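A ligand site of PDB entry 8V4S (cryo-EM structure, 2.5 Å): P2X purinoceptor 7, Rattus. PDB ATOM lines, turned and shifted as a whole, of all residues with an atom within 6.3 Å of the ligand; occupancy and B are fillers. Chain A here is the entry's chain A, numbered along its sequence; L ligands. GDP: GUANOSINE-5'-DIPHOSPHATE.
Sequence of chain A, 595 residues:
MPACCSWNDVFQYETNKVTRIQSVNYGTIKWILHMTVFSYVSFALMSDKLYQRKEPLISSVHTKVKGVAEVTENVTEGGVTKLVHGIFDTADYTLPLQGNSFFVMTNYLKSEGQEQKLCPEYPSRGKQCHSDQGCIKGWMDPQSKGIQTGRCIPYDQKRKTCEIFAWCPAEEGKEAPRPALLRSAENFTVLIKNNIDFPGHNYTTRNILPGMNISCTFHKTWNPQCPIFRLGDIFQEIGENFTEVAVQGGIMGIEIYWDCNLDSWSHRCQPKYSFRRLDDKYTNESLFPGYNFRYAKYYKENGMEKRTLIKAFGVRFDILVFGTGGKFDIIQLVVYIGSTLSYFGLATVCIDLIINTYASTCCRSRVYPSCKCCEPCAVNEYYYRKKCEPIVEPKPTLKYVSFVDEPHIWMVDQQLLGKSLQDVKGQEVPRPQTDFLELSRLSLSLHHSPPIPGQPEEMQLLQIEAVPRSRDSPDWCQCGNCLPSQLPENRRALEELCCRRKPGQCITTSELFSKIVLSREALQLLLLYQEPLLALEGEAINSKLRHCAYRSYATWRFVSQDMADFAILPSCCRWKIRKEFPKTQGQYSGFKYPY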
ATOM      1  N   GLU A 495      13.684 -20.359 -33.455  1.00  0.00           N
ATOM      2  CA  GLU A 495      14.961 -20.811 -32.927  1.00  0.00           C
ATOM      3  C   GLU A 495      15.807 -21.546 -33.963  1.00  0.00           C
ATOM      4  O   GLU A 495      16.868 -22.068 -33.619  1.00  0.00           O
ATOM      5  CB  GLU A 495      14.746 -21.697 -31.707  1.00  0.00           C
ATOM      6  CG  GLU A 495      14.094 -20.980 -30.538  1.00  0.00           C
ATOM      7  CD  GLU A 495      14.360 -21.661 -29.208  1.00  0.00           C
ATOM      8  OE1 GLU A 495      14.989 -22.739 -29.208  1.00  0.00           O
ATOM      9  OE2 GLU A 495      13.956 -21.109 -28.167  1.00  0.00           O
ATOM     10  N   SER A 543      19.152 -20.023 -13.730  1.00  0.00           N
ATOM     11  CA  SER A 543      18.313 -19.232 -14.638  1.00  0.00           C
ATOM     12  C   SER A 543      18.931 -17.861 -14.891  1.00  0.00           C
ATOM     13  O   SER A 543      18.981 -17.396 -16.044  1.00  0.00           O
ATOM     14  CB  SER A 543      16.902 -19.103 -14.064  1.00  0.00           C
ATOM     15  OG  SER A 543      16.094 -18.282 -14.882  1.00  0.00           O
ATOM     16  N   ARG A 546      21.961 -18.218 -17.112  1.00  0.00           N
ATOM     17  CA  ARG A 546      21.569 -18.354 -18.515  1.00  0.00           C
ATOM     18  C   ARG A 546      21.156 -17.012 -19.101  1.00  0.00           C
ATOM     19  O   ARG A 546      21.535 -16.683 -20.242  1.00  0.00           O
ATOM     20  CB  ARG A 546      20.416 -19.352 -18.645  1.00  0.00           C
ATOM     21  CG  ARG A 546      20.839 -20.787 -18.876  1.00  0.00           C
ATOM     22  CD  ARG A 546      19.686 -21.587 -19.442  1.00  0.00           C
ATOM     23  NE  ARG A 546      18.427 -21.264 -18.779  1.00  0.00           N
ATOM     24  CZ  ARG A 546      18.010 -21.817 -17.650  1.00  0.00           C
ATOM     25  NH1 ARG A 546      18.746 -22.742 -17.047  1.00  0.00           N
ATOM     26  NH2 ARG A 546      16.843 -21.459 -17.127  1.00  0.00           N
ATOM     27  N   HIS A 547      20.391 -16.228 -18.352  1.00  0.00           N
ATOM     28  CA  HIS A 547      19.987 -14.908 -18.833  1.00  0.00           C
ATOM     29  C   HIS A 547      21.203 -14.023 -19.076  1.00  0.00           C
ATOM     30  O   HIS A 547      21.298 -13.340 -20.104  1.00  0.00           O
ATOM     31  CB  HIS A 547      19.034 -14.245 -17.837  1.00  0.00           C
ATOM     32  CG  HIS A 547      17.719 -14.954 -17.690  1.00  0.00           C
ATOM     33  ND1 HIS A 547      17.495 -16.220 -18.185  1.00  0.00           N
ATOM     34  CD2 HIS A 547      16.569 -14.562 -17.104  1.00  0.00           C
ATOM     35  CE1 HIS A 547      16.257 -16.582 -17.912  1.00  0.00           C
ATOM     36  NE2 HIS A 547      15.671 -15.596 -17.261  1.00  0.00           N
ATOM     37  N   TYR A 550      23.088 -15.202 -22.244  1.00  0.00           N
ATOM     38  CA  TYR A 550      22.392 -14.721 -23.462  1.00  0.00           C
ATOM     39  C   TYR A 550      22.732 -13.245 -23.681  1.00  0.00           C
ATOM     40  O   TYR A 550      23.161 -12.885 -24.792  1.00  0.00           O
ATOM     41  CB  TYR A 550      20.872 -14.891 -23.360  1.00  0.00           C
ATOM     42  CG  TYR A 550      20.368 -16.294 -23.137  1.00  0.00           C
ATOM     43  CD1 TYR A 550      20.876 -17.365 -23.848  1.00  0.00           C
ATOM     44  CD2 TYR A 550      19.338 -16.539 -22.252  1.00  0.00           C
ATOM     45  CE1 TYR A 550      20.406 -18.653 -23.652  1.00  0.00           C
ATOM     46  CE2 TYR A 550      18.849 -17.822 -22.042  1.00  0.00           C
ATOM     47  CZ  TYR A 550      19.384 -18.881 -22.746  1.00  0.00           C
ATOM     48  OH  TYR A 550      18.913 -20.152 -22.544  1.00  0.00           O
ATOM     49  N   ARG A 551      22.529 -12.424 -22.649  1.00  0.00           N
ATOM     50  CA  ARG A 551      22.801 -10.962 -22.757  1.00  0.00           C
ATOM     51  C   ARG A 551      24.274 -10.737 -23.136  1.00  0.00           C
ATOM     52  O   ARG A 551      24.525  -9.927 -24.045  1.00  0.00           O
ATOM     53  CB  ARG A 551      22.508 -10.253 -21.436  1.00  0.00           C
ATOM     54  CG  ARG A 551      21.033 -10.131 -21.097  1.00  0.00           C
ATOM     55  CD  ARG A 551      20.829  -9.076 -20.024  1.00  0.00           C
ATOM     56  NE  ARG A 551      21.370  -7.793 -20.455  1.00  0.00           N
ATOM     57  CZ  ARG A 551      21.371  -6.683 -19.726  1.00  0.00           C
ATOM     58  NH1 ARG A 551      21.095  -6.742 -18.432  1.00  0.00           N
ATOM     59  NH2 ARG A 551      21.652  -5.518 -20.279  1.00  0.00           N
ATOM     60  N   ALA A 554      24.620 -11.370 -26.735  1.00  0.00           N
ATOM     61  CA  ALA A 554      23.949 -10.344 -27.525  1.00  0.00           C
ATOM     62  C   ALA A 554      24.737  -9.041 -27.512  1.00  0.00           C
ATOM     63  O   ALA A 554      24.878  -8.393 -28.549  1.00  0.00           O
ATOM     64  CB  ALA A 554      22.525 -10.123 -26.999  1.00  0.00           C
ATOM     65  N   MET A 563      19.657  -2.923 -30.224  1.00  0.00           N
ATOM     66  CA  MET A 563      19.653  -4.085 -31.102  1.00  0.00           C
ATOM     67  C   MET A 563      19.836  -5.392 -30.341  1.00  0.00           C
ATOM     68  O   MET A 563      19.303  -6.421 -30.768  1.00  0.00           O
ATOM     69  CB  MET A 563      20.752  -3.940 -32.157  1.00  0.00           C
ATOM     70  CG  MET A 563      20.355  -3.062 -33.329  1.00  0.00           C
ATOM     71  SD  MET A 563      21.464  -3.210 -34.742  1.00  0.00           S
ATOM     72  CE  MET A 563      22.964  -3.745 -33.926  1.00  0.00           C
ATOM     73  N   ALA A 564      20.577  -5.363 -29.230  1.00  0.00           N
ATOM     74  CA  ALA A 564      20.783  -6.579 -28.440  1.00  0.00           C
ATOM     75  C   ALA A 564      19.514  -7.032 -27.746  1.00  0.00           C
ATOM     76  O   ALA A 564      19.418  -8.213 -27.366  1.00  0.00           O
ATOM     77  CB  ALA A 564      21.890  -6.345 -27.409  1.00  0.00           C
ATOM     78  N   ASP A 565      18.536  -6.144 -27.556  1.00  0.00           N
ATOM     79  CA  ASP A 565      17.288  -6.539 -26.923  1.00  0.00           C
ATOM     80  C   ASP A 565      16.477  -7.479 -27.807  1.00  0.00           C
ATOM     81  O   ASP A 565      15.842  -8.415 -27.318  1.00  0.00           O
ATOM     82  CB  ASP A 565      16.466  -5.309 -26.558  1.00  0.00           C
ATOM     83  CG  ASP A 565      17.023  -4.557 -25.367  1.00  0.00           C
ATOM     84  OD1 ASP A 565      18.103  -4.956 -24.874  1.00  0.00           O
ATOM     85  OD2 ASP A 565      16.394  -3.575 -24.924  1.00  0.00           O
ATOM     86  N   PHE A 566      16.486  -7.232 -29.115  1.00  0.00           N
ATOM     87  CA  PHE A 566      15.745  -8.048 -30.071  1.00  0.00           C
ATOM     88  C   PHE A 566      16.619  -9.023 -30.824  1.00  0.00           C
ATOM     89  O   PHE A 566      16.140  -9.697 -31.749  1.00  0.00           O
ATOM     90  CB  PHE A 566      14.991  -7.134 -31.045  1.00  0.00           C
ATOM     91  CG  PHE A 566      13.925  -6.308 -30.394  1.00  0.00           C
ATOM     92  CD1 PHE A 566      14.221  -5.065 -29.871  1.00  0.00           C
ATOM     93  CD2 PHE A 566      12.637  -6.789 -30.293  1.00  0.00           C
ATOM     94  CE1 PHE A 566      13.241  -4.313 -29.261  1.00  0.00           C
ATOM     95  CE2 PHE A 566      11.652  -6.031 -29.687  1.00  0.00           C
ATOM     96  CZ  PHE A 566      11.957  -4.796 -29.169  1.00  0.00           C
ATOM     97  N   ALA A 567      17.896  -9.131 -30.454  1.00  0.00           N
ATOM     98  CA  ALA A 567      18.789 -10.097 -31.085  1.00  0.00           C
ATOM     99  C   ALA A 567      18.382 -11.516 -30.728  1.00  0.00           C
ATOM    100  O   ALA A 567      17.904 -11.793 -29.622  1.00  0.00           O
ATOM    101  CB  ALA A 567      20.226  -9.841 -30.641  1.00  0.00           C
ATOM    102  N   ILE A 568      18.577 -12.428 -31.677  1.00  0.00           N
ATOM    103  CA  ILE A 568      18.234 -13.835 -31.508  1.00  0.00           C
ATOM    104  C   ILE A 568      19.511 -14.648 -31.563  1.00  0.00           C
ATOM    105  O   ILE A 568      20.288 -14.534 -32.522  1.00  0.00           O
ATOM    106  CB  ILE A 568      17.229 -14.309 -32.568  1.00  0.00           C
ATOM    107  CG1 ILE A 568      16.108 -13.283 -32.750  1.00  0.00           C
ATOM    108  CG2 ILE A 568      16.648 -15.662 -32.177  1.00  0.00           C
ATOM    109  CD1 ILE A 568      15.211 -13.133 -31.548  1.00  0.00           C
ATOM    110  N   LEU A 569      19.728 -15.475 -30.538  1.00  0.00           N
ATOM    111  CA  LEU A 569      20.914 -16.321 -30.475  1.00  0.00           C
ATOM    112  C   LEU A 569      20.780 -17.497 -31.436  1.00  0.00           C
ATOM    113  O   LEU A 569      19.684 -18.051 -31.600  1.00  0.00           O
ATOM    114  CB  LEU A 569      21.119 -16.841 -29.063  1.00  0.00           C
ATOM    115  CG  LEU A 569      22.036 -16.034 -28.145  1.00  0.00           C
ATOM    116  CD1 LEU A 569      21.371 -14.748 -27.689  1.00  0.00           C
ATOM    117  CD2 LEU A 569      22.457 -16.880 -26.952  1.00  0.00           C
ATOM    118  N   PRO A 570      21.865 -17.898 -32.096  1.00  0.00           N
ATOM    119  CA  PRO A 570      21.835 -19.133 -32.879  1.00  0.00           C
ATOM    120  C   PRO A 570      21.716 -20.364 -31.988  1.00  0.00           C
ATOM    121  O   PRO A 570      21.964 -20.315 -30.784  1.00  0.00           O
ATOM    122  CB  PRO A 570      23.174 -19.119 -33.630  1.00  0.00           C
ATOM    123  CG  PRO A 570      24.035 -18.206 -32.852  1.00  0.00           C
ATOM    124  CD  PRO A 570      23.141 -17.178 -32.237  1.00  0.00           C
ATOM    125  N   ARG A 574      22.985 -21.071 -28.076  1.00  0.00           N
ATOM    126  CA  ARG A 574      21.896 -21.232 -27.123  1.00  0.00           C
ATOM    127  C   ARG A 574      22.007 -22.560 -26.391  1.00  0.00           C
ATOM    128  O   ARG A 574      21.905 -22.610 -25.150  1.00  0.00           O
ATOM    129  CB  ARG A 574      20.561 -21.136 -27.855  1.00  0.00           C
ATOM    130  CG  ARG A 574      19.338 -21.362 -26.994  1.00  0.00           C
ATOM    131  CD  ARG A 574      18.083 -21.443 -27.841  1.00  0.00           C
ATOM    132  NE  ARG A 574      18.040 -20.405 -28.859  1.00  0.00           N
ATOM    133  CZ  ARG A 574      17.619 -19.163 -28.646  1.00  0.00           C
ATOM    134  NH1 ARG A 574      17.193 -18.799 -27.437  1.00  0.00           N
ATOM    135  NH2 ARG A 574      17.616 -18.275 -29.636  1.00  0.00           N
ATOM    136  N   ARG A 578      22.776 -23.505 -22.512  1.00  0.00           N
ATOM    137  CA  ARG A 578      21.845 -24.303 -21.732  1.00  0.00           C
ATOM    138  C   ARG A 578      22.464 -25.608 -21.227  1.00  0.00           C
ATOM    139  O   ARG A 578      22.016 -26.130 -20.203  1.00  0.00           O
ATOM    140  CB  ARG A 578      20.594 -24.598 -22.559  1.00  0.00           C
ATOM    141  CG  ARG A 578      19.733 -23.362 -22.770  1.00  0.00           C
ATOM    142  CD  ARG A 578      18.662 -23.573 -23.817  1.00  0.00           C
ATOM    143  NE  ARG A 578      17.797 -22.406 -23.906  1.00  0.00           N
ATOM    144  CZ  ARG A 578      16.774 -22.295 -24.744  1.00  0.00           C
ATOM    145  NH1 ARG A 578      16.491 -23.280 -25.584  1.00  0.00           N
ATOM    146  NH2 ARG A 578      16.040 -21.190 -24.763  1.00  0.00           N
ATOM    147  N   LYS A 583      18.436 -26.164 -16.623  1.00  0.00           N
ATOM    148  CA  LYS A 583      17.337 -25.957 -15.685  1.00  0.00           C
ATOM    149  C   LYS A 583      16.704 -27.296 -15.315  1.00  0.00           C
ATOM    150  O   LYS A 583      16.762 -28.259 -16.080  1.00  0.00           O
ATOM    151  CB  LYS A 583      16.281 -25.014 -16.268  1.00  0.00           C
ATOM    152  CG  LYS A 583      15.283 -25.687 -17.202  1.00  0.00           C
ATOM    153  CD  LYS A 583      14.321 -24.679 -17.814  1.00  0.00           C
ATOM    154  CE  LYS A 583      13.689 -23.796 -16.743  1.00  0.00           C
ATOM    155  NZ  LYS A 583      12.824 -24.579 -15.826  1.00  0.00           N
ATOM    156  N   GLY A 586      11.573 -28.297 -16.170  1.00  0.00           N
ATOM    157  CA  GLY A 586      10.934 -27.211 -16.899  1.00  0.00           C
ATOM    158  C   GLY A 586      11.343 -27.218 -18.349  1.00  0.00           C
ATOM    159  O   GLY A 586      12.193 -28.013 -18.776  1.00  0.00           O
ATOM    160  N   GLN A 587      10.717 -26.320 -19.104  1.00  0.00           N
ATOM    161  CA  GLN A 587      11.012 -26.119 -20.513  1.00  0.00           C
ATOM    162  C   GLN A 587      11.483 -24.698 -20.729  1.00  0.00           C
ATOM    163  O   GLN A 587      10.932 -23.754 -20.164  1.00  0.00           O
ATOM    164  CB  GLN A 587       9.785 -26.404 -21.388  1.00  0.00           C
ATOM    165  CG  GLN A 587       9.239 -27.823 -21.261  1.00  0.00           C
ATOM    166  CD  GLN A 587       8.043 -28.064 -22.159  1.00  0.00           C
ATOM    167  OE1 GLN A 587       7.673 -27.215 -22.969  1.00  0.00           O
ATOM    168  NE2 GLN A 587       7.420 -29.225 -22.011  1.00  0.00           N
ATOM    169  N   TYR A 588      12.517 -24.536 -21.561  1.00  0.00           N
ATOM    170  CA  TYR A 588      13.082 -23.225 -21.818  1.00  0.00           C
ATOM    171  C   TYR A 588      12.085 -22.354 -22.581  1.00  0.00           C
ATOM    172  O   TYR A 588      11.520 -22.778 -23.594  1.00  0.00           O
ATOM    173  CB  TYR A 588      14.386 -23.362 -22.608  1.00  0.00           C
ATOM    174  CG  TYR A 588      15.412 -24.239 -21.932  1.00  0.00           C
ATOM    175  CD1 TYR A 588      16.237 -23.741 -20.937  1.00  0.00           C
ATOM    176  CD2 TYR A 588      15.551 -25.574 -22.290  1.00  0.00           C
ATOM    177  CE1 TYR A 588      17.179 -24.536 -20.319  1.00  0.00           C
ATOM    178  CE2 TYR A 588      16.495 -26.385 -21.678  1.00  0.00           C
ATOM    179  CZ  TYR A 588      17.302 -25.866 -20.695  1.00  0.00           C
ATOM    180  OH  TYR A 588      18.244 -26.661 -20.076  1.00  0.00           O
ATOM    181  N   SER A 589      11.886 -21.133 -22.096  1.00  0.00           N
ATOM    182  CA  SER A 589      10.876 -20.252 -22.682  1.00  0.00           C
ATOM    183  C   SER A 589      11.340 -19.626 -23.995  1.00  0.00           C
ATOM    184  O   SER A 589      10.515 -19.398 -24.883  1.00  0.00           O
ATOM    185  CB  SER A 589      10.504 -19.154 -21.684  1.00  0.00           C
ATOM    186  OG  SER A 589      11.614 -18.318 -21.411  1.00  0.00           O
ATOM    187  N   GLY A 590      12.635 -19.356 -24.130  1.00  0.00           N
ATOM    188  CA  GLY A 590      13.139 -18.725 -25.335  1.00  0.00           C
ATOM    189  C   GLY A 590      13.022 -17.214 -25.303  1.00  0.00           C
ATOM    190  O   GLY A 590      12.774 -16.596 -24.258  1.00  0.00           O
ATOM    191  N   PHE A 591      13.214 -16.620 -26.471  1.00  0.00           N
ATOM    192  CA  PHE A 591      13.140 -15.167 -26.594  1.00  0.00           C
ATOM    193  C   PHE A 591      11.740 -14.668 -26.257  1.00  0.00           C
ATOM    194  O   PHE A 591      10.738 -15.263 -26.682  1.00  0.00           O
ATOM    195  CB  PHE A 591      13.536 -14.736 -28.003  1.00  0.00           C
ATOM    196  CG  PHE A 591      13.387 -13.260 -28.253  1.00  0.00           C
ATOM    197  CD1 PHE A 591      14.154 -12.339 -27.551  1.00  0.00           C
ATOM    198  CD2 PHE A 591      12.476 -12.786 -29.184  1.00  0.00           C
ATOM    199  CE1 PHE A 591      14.006 -10.987 -27.772  1.00  0.00           C
ATOM    200  CE2 PHE A 591      12.328 -11.434 -29.404  1.00  0.00           C
ATOM    201  CZ  PHE A 591      13.094 -10.528 -28.699  1.00  0.00           C
ATOM    202  N   LYS A 592      11.688 -13.597 -25.461  1.00  0.00           N
ATOM    203  CA  LYS A 592      10.395 -12.999 -25.058  1.00  0.00           C
ATOM    204  C   LYS A 592      10.409 -11.510 -25.419  1.00  0.00           C
ATOM    205  O   LYS A 592      11.483 -10.893 -25.343  1.00  0.00           O
ATOM    206  CB  LYS A 592      10.188 -13.202 -23.555  1.00  0.00           C
ATOM    207  CG  LYS A 592       9.032 -12.439 -22.930  1.00  0.00           C
ATOM    208  CD  LYS A 592       8.991 -12.556 -21.426  1.00  0.00           C
ATOM    209  CE  LYS A 592      10.302 -12.202 -20.777  1.00  0.00           C
ATOM    210  NZ  LYS A 592      10.271 -12.414 -19.312  1.00  0.00           N
HETATM  211  PB  GDP L   1      14.040 -20.291 -18.382  1.00  0.00           P
HETATM  212  O1B GDP L   1      14.456 -20.640 -16.964  1.00  0.00           O
HETATM  213  O2B GDP L   1      12.976 -19.233 -18.348  1.00  0.00           O
HETATM  214  O3B GDP L   1      13.503 -21.520 -19.075  1.00  0.00           O
HETATM  215  O3A GDP L   1      15.324 -19.739 -19.181  1.00  0.00           O
HETATM  216  PA  GDP L   1      15.152 -19.284 -20.718  1.00  0.00           P
HETATM  217  O1A GDP L   1      16.150 -19.979 -21.605  1.00  0.00           O
HETATM  218  O2A GDP L   1      13.738 -19.533 -21.188  1.00  0.00           O
HETATM  219  O5' GDP L   1      15.449 -17.708 -20.651  1.00  0.00           O
HETATM  220  C5' GDP L   1      14.516 -16.795 -21.219  1.00  0.00           C
HETATM  221  C4' GDP L   1      15.088 -15.394 -21.182  1.00  0.00           C
HETATM  222  O4' GDP L   1      16.268 -15.366 -21.966  1.00  0.00           O
HETATM  223  C3' GDP L   1      14.101 -14.404 -21.786  1.00  0.00           C
HETATM  224  O3' GDP L   1      13.824 -13.357 -20.853  1.00  0.00           O
HETATM  225  C2' GDP L   1      14.768 -13.844 -23.017  1.00  0.00           C
HETATM  226  O2' GDP L   1      14.751 -12.412 -22.976  1.00  0.00           O
HETATM  227  C1' GDP L   1      16.205 -14.353 -22.973  1.00  0.00           C
HETATM  228  N9  GDP L   1      16.564 -14.928 -24.283  1.00  0.00           N
HETATM  229  C8  GDP L   1      16.495 -16.233 -24.620  1.00  0.00           C
HETATM  230  N7  GDP L   1      16.890 -16.420 -25.903  1.00  0.00           N
HETATM  231  C5  GDP L   1      17.215 -15.220 -26.407  1.00  0.00           C
HETATM  232  C6  GDP L   1      17.699 -14.707 -27.697  1.00  0.00           C
HETATM  233  O6  GDP L   1      17.917 -15.480 -28.661  1.00  0.00           O
HETATM  234  N1  GDP L   1      17.918 -13.394 -27.810  1.00  0.00           N
HETATM  235  C2  GDP L   1      17.699 -12.537 -26.791  1.00  0.00           C
HETATM  236  N2  GDP L   1      17.940 -11.223 -26.993  1.00  0.00           N
HETATM  237  N3  GDP L   1      17.243 -12.940 -25.582  1.00  0.00           N
HETATM  238  C4  GDP L   1      16.997 -14.238 -25.342  1.00  0.00           C
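O of Ala 567 sits at hydrogen-bond distance from N1 of the ligand, 2.4 Å away. An oxygen (O2A) of the ligand sits at hydrogen-bond distance from the backbone NH of Ser 589 (2.6 Å). OG of Ser 589 lies within hydrogen-bond range of O2A of the ligand, at 2.5 Å. NH2 of Arg 546 is in salt-bridge range of O1B of the ligand (2.5 Å). An oxygen (O6) of the ligand is in hydrogen-bond range of the backbone NH of Leu 569 (2.6 Å). A nitrogen (N7) of the ligand is in hydrogen-bond range of the guanidinium group (NH1) of Arg 574, 2.8 Å away. An oxygen (O1A) of the ligand sits at hydrogen-bond distance from the side-chain hydroxyl (OH) of Tyr 550 (2.9 Å). The backbone NH (N) of Gly 590 sits at hydrogen-bond distance from an oxygen (O2A) of the ligand, 3.1 Å away. O of Ala 564 lies within hydrogen-bond range of N2 of the ligand (3.4 Å). The guanidinium group of Arg 578 is in salt-bridge range of an oxygen (O1A) of the ligand, 3.4 Å away.
Merely in contact with the ligand: Ser 543 (3.5 Å), His 547 (3.1 Å), Asp 565 (3.5 Å), Ile 568 (3.3 Å), Lys 583 (3.3 Å), Gln 587 (3.6 Å), Tyr 588 (3.3 Å), Phe 591 (3.6 Å) and Lys 592 (3.7 Å). Hydrophobic or aromatic side chains that line the ligand: His 547, Tyr 550, Ile 568, Leu 569, Tyr 588 and Phe 591. 18 residues have an atom within 4 Å of the ligand: Ser 543, Arg 546, His 547, Tyr 550, Ala 564, Asp 565, Ala 567, Ile 568, Leu 569, Arg 574, Arg 578, Lys 583, Gln 587, Tyr 588, Ser 589, Gly 590, Phe 591 and Lys 592. The nearest printed residue that does not touch the ligand is Phe 566 (4.6 Å).
The guanidinium group (NH2) of Arg 574 is in hydrogen-bond range of the backbone carbonyl oxygen (O) of Leu 569 (2.9 Å). NE of Arg 574 lies within salt-bridge range of OE1 of Glu 495 (3.9 Å). The side-chain hydroxyl (OH) of Tyr 550 sits at hydrogen-bond distance from the guanidinium group (NE) of Arg 578 (2.9 Å). A ring nitrogen (ND1) of His 547 sits at hydrogen-bond distance from the backbone carbonyl oxygen (O) of Ser 543, at 2.9 Å. The side-chain hydroxyl (OH) of Tyr 588 lies within hydrogen-bond range of the backbone NH (N) of Lys 583 (3.5 Å). OE1 of Glu 495 is in salt-bridge range of NH1 of Arg 578 (3.96 Å).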
